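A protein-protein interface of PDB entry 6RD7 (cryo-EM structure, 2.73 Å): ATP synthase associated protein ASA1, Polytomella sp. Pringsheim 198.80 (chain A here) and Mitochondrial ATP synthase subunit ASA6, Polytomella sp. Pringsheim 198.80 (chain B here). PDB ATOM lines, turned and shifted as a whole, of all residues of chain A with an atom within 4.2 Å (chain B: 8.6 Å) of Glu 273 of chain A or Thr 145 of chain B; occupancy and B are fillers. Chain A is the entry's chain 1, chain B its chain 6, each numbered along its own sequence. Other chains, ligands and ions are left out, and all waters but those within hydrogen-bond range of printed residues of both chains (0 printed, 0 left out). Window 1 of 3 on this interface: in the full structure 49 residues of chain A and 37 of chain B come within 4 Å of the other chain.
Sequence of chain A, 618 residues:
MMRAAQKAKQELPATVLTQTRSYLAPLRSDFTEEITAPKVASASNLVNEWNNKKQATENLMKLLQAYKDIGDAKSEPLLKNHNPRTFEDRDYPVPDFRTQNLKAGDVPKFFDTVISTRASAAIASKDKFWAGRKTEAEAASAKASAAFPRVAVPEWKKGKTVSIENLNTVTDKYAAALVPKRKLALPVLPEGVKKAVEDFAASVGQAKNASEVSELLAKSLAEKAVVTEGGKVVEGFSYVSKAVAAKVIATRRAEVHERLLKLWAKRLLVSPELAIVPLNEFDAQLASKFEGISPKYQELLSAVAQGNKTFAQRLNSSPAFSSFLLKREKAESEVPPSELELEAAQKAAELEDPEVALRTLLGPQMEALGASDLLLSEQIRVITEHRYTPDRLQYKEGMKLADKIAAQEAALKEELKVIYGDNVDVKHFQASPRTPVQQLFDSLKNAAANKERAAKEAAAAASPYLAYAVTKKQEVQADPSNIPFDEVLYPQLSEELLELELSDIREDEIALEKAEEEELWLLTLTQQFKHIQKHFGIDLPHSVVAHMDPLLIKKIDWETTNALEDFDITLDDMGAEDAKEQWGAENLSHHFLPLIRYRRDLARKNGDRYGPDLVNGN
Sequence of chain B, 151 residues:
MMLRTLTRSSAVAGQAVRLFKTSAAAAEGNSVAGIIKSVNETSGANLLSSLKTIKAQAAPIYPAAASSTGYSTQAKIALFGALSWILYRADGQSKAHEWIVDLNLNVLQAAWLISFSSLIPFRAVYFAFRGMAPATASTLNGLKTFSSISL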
ATOM      1  N   SER A 271     -15.510 -14.080  20.200  1.00  0.00           N
ATOM      2  CA  SER A 271     -16.041 -15.428  20.060  1.00  0.00           C
ATOM      3  C   SER A 271     -14.949 -16.410  19.656  1.00  0.00           C
ATOM      4  O   SER A 271     -14.652 -16.548  18.464  1.00  0.00           O
ATOM      5  CB  SER A 271     -17.171 -15.441  19.036  1.00  0.00           C
ATOM      6  OG  SER A 271     -16.701 -15.063  17.760  1.00  0.00           O
ATOM      7  N   PRO A 272     -14.344 -17.127  20.611  1.00  0.00           N
ATOM      8  CA  PRO A 272     -13.226 -18.022  20.273  1.00  0.00           C
ATOM      9  C   PRO A 272     -13.635 -19.289  19.547  1.00  0.00           C
ATOM     10  O   PRO A 272     -12.752 -19.982  19.017  1.00  0.00           O
ATOM     11  CB  PRO A 272     -12.619 -18.351  21.638  1.00  0.00           C
ATOM     12  CG  PRO A 272     -13.726 -18.160  22.594  1.00  0.00           C
ATOM     13  CD  PRO A 272     -14.549 -17.034  22.064  1.00  0.00           C
ATOM     14  N   GLU A 273     -14.935 -19.594  19.472  1.00  0.00           N
ATOM     15  CA  GLU A 273     -15.426 -20.789  18.794  1.00  0.00           C
ATOM     16  C   GLU A 273     -15.105 -20.801  17.306  1.00  0.00           C
ATOM     17  O   GLU A 273     -15.034 -21.887  16.730  1.00  0.00           O
ATOM     18  CB  GLU A 273     -16.934 -20.937  19.001  1.00  0.00           C
ATOM     19  CG  GLU A 273     -17.789 -19.958  18.222  1.00  0.00           C
ATOM     20  CD  GLU A 273     -18.272 -18.811  19.076  1.00  0.00           C
ATOM     21  OE1 GLU A 273     -17.766 -18.657  20.205  1.00  0.00           O
ATOM     22  OE2 GLU A 273     -19.165 -18.066  18.621  1.00  0.00           O
ATOM     23  N   LEU A 274     -14.799 -19.638  16.711  1.00  0.00           N
ATOM     24  CA  LEU A 274     -14.343 -19.553  15.324  1.00  0.00           C
ATOM     25  C   LEU A 274     -13.062 -20.350  15.085  1.00  0.00           C
ATOM     26  O   LEU A 274     -12.748 -20.700  13.943  1.00  0.00           O
ATOM     27  CB  LEU A 274     -14.119 -18.088  14.946  1.00  0.00           C
ATOM     28  CG  LEU A 274     -15.210 -17.297  14.229  1.00  0.00           C
ATOM     29  CD1 LEU A 274     -16.433 -17.140  15.102  1.00  0.00           C
ATOM     30  CD2 LEU A 274     -14.672 -15.939  13.829  1.00  0.00           C
ATOM     31  N   ALA A 275     -12.312 -20.655  16.149  1.00  0.00           N
ATOM     32  CA  ALA A 275     -11.106 -21.453  16.002  1.00  0.00           C
ATOM     33  C   ALA A 275     -11.384 -22.935  15.766  1.00  0.00           C
ATOM     34  O   ALA A 275     -10.438 -23.682  15.501  1.00  0.00           O
ATOM     35  CB  ALA A 275     -10.223 -21.284  17.236  1.00  0.00           C
ATOM     36  N   ILE A 276     -12.637 -23.400  15.853  1.00  0.00           N
ATOM     37  CA  ILE A 276     -12.855 -24.830  15.644  1.00  0.00           C
ATOM     38  C   ILE A 276     -13.125 -25.125  14.175  1.00  0.00           C
ATOM     39  O   ILE A 276     -13.074 -26.281  13.743  1.00  0.00           O
ATOM     40  CB  ILE A 276     -13.987 -25.369  16.537  1.00  0.00           C
ATOM     41  CG1 ILE A 276     -15.348 -24.973  15.989  1.00  0.00           C
ATOM     42  CG2 ILE A 276     -13.832 -24.856  17.933  1.00  0.00           C
ATOM     43  CD1 ILE A 276     -16.477 -25.570  16.723  1.00  0.00           C
ATOM     44  N   LEU A 301     -20.321 -25.664  16.651  1.00  0.00           N
ATOM     45  CA  LEU A 301     -19.977 -24.257  16.873  1.00  0.00           C
ATOM     46  C   LEU A 301     -20.898 -23.618  17.896  1.00  0.00           C
ATOM     47  O   LEU A 301     -20.435 -22.956  18.835  1.00  0.00           O
ATOM     48  CB  LEU A 301     -20.058 -23.503  15.554  1.00  0.00           C
ATOM     49  CG  LEU A 301     -19.336 -22.216  15.230  1.00  0.00           C
ATOM     50  CD1 LEU A 301     -17.876 -22.417  15.268  1.00  0.00           C
ATOM     51  CD2 LEU A 301     -19.712 -21.915  13.828  1.00  0.00           C
ATOM     52  N   VAL A 304     -20.033 -25.044  21.285  1.00  0.00           N
ATOM     53  CA  VAL A 304     -18.830 -24.494  21.894  1.00  0.00           C
ATOM     54  C   VAL A 304     -19.081 -23.057  22.352  1.00  0.00           C
ATOM     55  O   VAL A 304     -18.470 -22.584  23.321  1.00  0.00           O
ATOM     56  CB  VAL A 304     -17.656 -24.645  20.898  1.00  0.00           C
ATOM     57  CG1 VAL A 304     -16.431 -23.825  21.266  1.00  0.00           C
ATOM     58  CG2 VAL A 304     -17.232 -26.091  20.816  1.00  0.00           C
ATOM     59  N   ALA A 305     -20.052 -22.375  21.736  1.00  0.00           N
ATOM     60  CA  ALA A 305     -20.284 -20.961  22.033  1.00  0.00           C
ATOM     61  C   ALA A 305     -20.907 -20.728  23.412  1.00  0.00           C
ATOM     62  O   ALA A 305     -20.951 -19.586  23.884  1.00  0.00           O
ATOM     63  CB  ALA A 305     -21.164 -20.346  20.949  1.00  0.00           C
ATOM     64  N   LYS A 530     -24.568 -14.053  22.588  1.00  0.00           N
ATOM     65  CA  LYS A 530     -23.815 -15.109  23.242  1.00  0.00           C
ATOM     66  C   LYS A 530     -23.991 -15.051  24.750  1.00  0.00           C
ATOM     67  O   LYS A 530     -24.194 -16.084  25.397  1.00  0.00           O
ATOM     68  CB  LYS A 530     -22.349 -14.978  22.851  1.00  0.00           C
ATOM     69  CG  LYS A 530     -21.511 -16.201  23.048  1.00  0.00           C
ATOM     70  CD  LYS A 530     -20.095 -15.908  22.615  1.00  0.00           C
ATOM     71  CE  LYS A 530     -19.147 -16.963  23.117  1.00  0.00           C
ATOM     72  NZ  LYS A 530     -17.738 -16.548  22.977  1.00  0.00           N
ATOM     73  N   GLY B 142     -31.463 -18.718  18.302  1.00  0.00           N
ATOM     74  CA  GLY B 142     -31.520 -17.420  17.674  1.00  0.00           C
ATOM     75  C   GLY B 142     -30.445 -17.219  16.635  1.00  0.00           C
ATOM     76  O   GLY B 142     -30.361 -17.952  15.648  1.00  0.00           O
ATOM     77  N   LEU B 143     -29.678 -16.150  16.836  1.00  0.00           N
ATOM     78  CA  LEU B 143     -28.508 -15.835  16.030  1.00  0.00           C
ATOM     79  C   LEU B 143     -27.521 -16.996  15.967  1.00  0.00           C
ATOM     80  O   LEU B 143     -27.061 -17.503  16.990  1.00  0.00           O
ATOM     81  CB  LEU B 143     -27.829 -14.602  16.617  1.00  0.00           C
ATOM     82  CG  LEU B 143     -26.444 -14.228  16.117  1.00  0.00           C
ATOM     83  CD1 LEU B 143     -26.565 -13.862  14.696  1.00  0.00           C
ATOM     84  CD2 LEU B 143     -25.887 -13.066  16.902  1.00  0.00           C
ATOM     85  N   LYS B 144     -27.208 -17.421  14.749  1.00  0.00           N
ATOM     86  CA  LYS B 144     -26.188 -18.424  14.499  1.00  0.00           C
ATOM     87  C   LYS B 144     -24.859 -17.735  14.240  1.00  0.00           C
ATOM     88  O   LYS B 144     -24.814 -16.551  13.902  1.00  0.00           O
ATOM     89  CB  LYS B 144     -26.550 -19.305  13.305  1.00  0.00           C
ATOM     90  CG  LYS B 144     -27.781 -20.153  13.502  1.00  0.00           C
ATOM     91  CD  LYS B 144     -27.640 -21.052  14.706  1.00  0.00           C
ATOM     92  CE  LYS B 144     -28.942 -21.762  14.996  1.00  0.00           C
ATOM     93  NZ  LYS B 144     -30.097 -20.826  14.930  1.00  0.00           N
ATOM     94  N   THR B 145     -23.773 -18.490  14.393  1.00  0.00           N
ATOM     95  CA  THR B 145     -22.447 -17.901  14.261  1.00  0.00           C
ATOM     96  C   THR B 145     -22.121 -17.584  12.806  1.00  0.00           C
ATOM     97  O   THR B 145     -21.577 -16.517  12.507  1.00  0.00           O
ATOM     98  CB  THR B 145     -21.406 -18.842  14.865  1.00  0.00           C
ATOM     99  OG1 THR B 145     -21.670 -19.017  16.261  1.00  0.00           O
ATOM    100  CG2 THR B 145     -20.002 -18.292  14.704  1.00  0.00           C
ATOM    101  N   PHE B 146     -22.514 -18.473  11.886  1.00  0.00           N
ATOM    102  CA  PHE B 146     -22.101 -18.365  10.487  1.00  0.00           C
ATOM    103  C   PHE B 146     -22.713 -17.156   9.790  1.00  0.00           C
ATOM    104  O   PHE B 146     -22.175 -16.679   8.786  1.00  0.00           O
ATOM    105  CB  PHE B 146     -22.480 -19.636   9.734  1.00  0.00           C
ATOM    106  CG  PHE B 146     -21.352 -20.608   9.563  1.00  0.00           C
ATOM    107  CD1 PHE B 146     -20.542 -20.560   8.446  1.00  0.00           C
ATOM    108  CD2 PHE B 146     -21.108 -21.575  10.515  1.00  0.00           C
ATOM    109  CE1 PHE B 146     -19.513 -21.465   8.285  1.00  0.00           C
ATOM    110  CE2 PHE B 146     -20.086 -22.486  10.351  1.00  0.00           C
ATOM    111  CZ  PHE B 146     -19.283 -22.424   9.243  1.00  0.00           C
ATOM    112  N   SER B 147     -23.839 -16.649  10.294  1.00  0.00           N
ATOM    113  CA  SER B 147     -24.427 -15.455   9.696  1.00  0.00           C
ATOM    114  C   SER B 147     -23.736 -14.193  10.189  1.00  0.00           C
ATOM    115  O   SER B 147     -23.697 -13.181   9.482  1.00  0.00           O
ATOM    116  CB  SER B 147     -25.920 -15.394   9.993  1.00  0.00           C
ATOM    117  OG  SER B 147     -26.151 -15.232  11.375  1.00  0.00           O
ATOM    118  N   SER B 148     -23.184 -14.231  11.397  1.00  0.00           N
ATOM    119  CA  SER B 148     -22.583 -13.062  12.020  1.00  0.00           C
ATOM    120  C   SER B 148     -21.062 -13.109  12.030  1.00  0.00           C
ATOM    121  O   SER B 148     -20.442 -12.426  12.849  1.00  0.00           O
ATOM    122  CB  SER B 148     -23.099 -12.907  13.449  1.00  0.00           C
ATOM    123  OG  SER B 148     -22.579 -13.923  14.283  1.00  0.00           O
ATOM    124  N   ILE B 149     -20.449 -13.906  11.153  1.00  0.00           N
ATOM    125  CA  ILE B 149     -18.996 -13.941  11.077  1.00  0.00           C
ATOM    126  C   ILE B 149     -18.495 -12.671  10.410  1.00  0.00           C
ATOM    127  O   ILE B 149     -18.950 -12.290   9.325  1.00  0.00           O
ATOM    128  CB  ILE B 149     -18.526 -15.204  10.334  1.00  0.00           C
ATOM    129  CG1 ILE B 149     -18.578 -16.406  11.270  1.00  0.00           C
ATOM    130  CG2 ILE B 149     -17.115 -15.054   9.808  1.00  0.00           C
ATOM    131  CD1 ILE B 149     -18.361 -17.717  10.589  1.00  0.00           C
ATOM    132  N   SER B 150     -17.559 -11.996  11.072  1.00  0.00           N
ATOM    133  CA  SER B 150     -16.975 -10.760  10.579  1.00  0.00           C
ATOM    134  C   SER B 150     -15.587 -11.040  10.026  1.00  0.00           C
ATOM    135  O   SER B 150     -14.706 -11.479  10.768  1.00  0.00           O
ATOM    136  CB  SER B 150     -16.890  -9.712  11.691  1.00  0.00           C
ATOM    137  OG  SER B 150     -16.264  -8.533  11.221  1.00  0.00           O
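No residue of chain B comes within 4 Å of Pro 272 of chain A.
Glu 273 of chain A touches just one residue of chain B: Thr 145.
Of the printed residues of chain B, Leu 274 of chain A touches Thr 145.
Printed residues of chain B within 4 Å of Leu 301 of chain A: Thr 145 (3.7 Å) and Phe 146 (3.5 Å).
Thr 145 of chain B touches just these residues of chain A: Glu 273, Leu 274 and Leu 301.
Of the printed residues of chain A, Phe 146 of chain B touches Leu 301.
The nearest residue of chain B that does not touch Glu 273 of chain A is Ser 148 of chain B (6.9 Å).
The nearest printed residue of chain A that does not touch Phe 146 of chain B is Leu 274 of chain A (7.0 Å).
Among the printed residues, merely in contact across the chains: Leu 301 of chain A with Phe 146 of chain B (3.5 Å), Glu 273 of chain A with Thr 145 of chain B (3.6 Å), Leu 301 of chain A with Thr 145 of chain B (3.7 Å) and Leu 274 of chain A with Thr 145 of chain B (3.8 Å).
Of the 10 printed residues of chain A, 3 touch a printed residue of chain B.
Hydrophobic or aromatic side chains of chain A that line the printed part of chain B: Leu 274 and Leu 301.
Printed residues of chain B that touch a printed residue of chain A: Thr 145 and Phe 146.
Hydrophobic or aromatic side chains of chain B within 4 Å of the printed part of chain A: Phe 146.
Among the printed residues, no Asp or Glu carboxylate lies within 4 Å of a Lys or Arg side-chain nitrogen of the other chain.
The side-chain carboxylate of Glu 273 of chain A is in salt-bridge range of the side-chain amino group of Lys 530 of chain A, 3.5 Å away.
The side-chain hydroxyl (OG) of Ser 148 of chain B is in hydrogen-bond range of the backbone carbonyl oxygen (O) of Thr 145 of chain B, 3.3 Å away.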
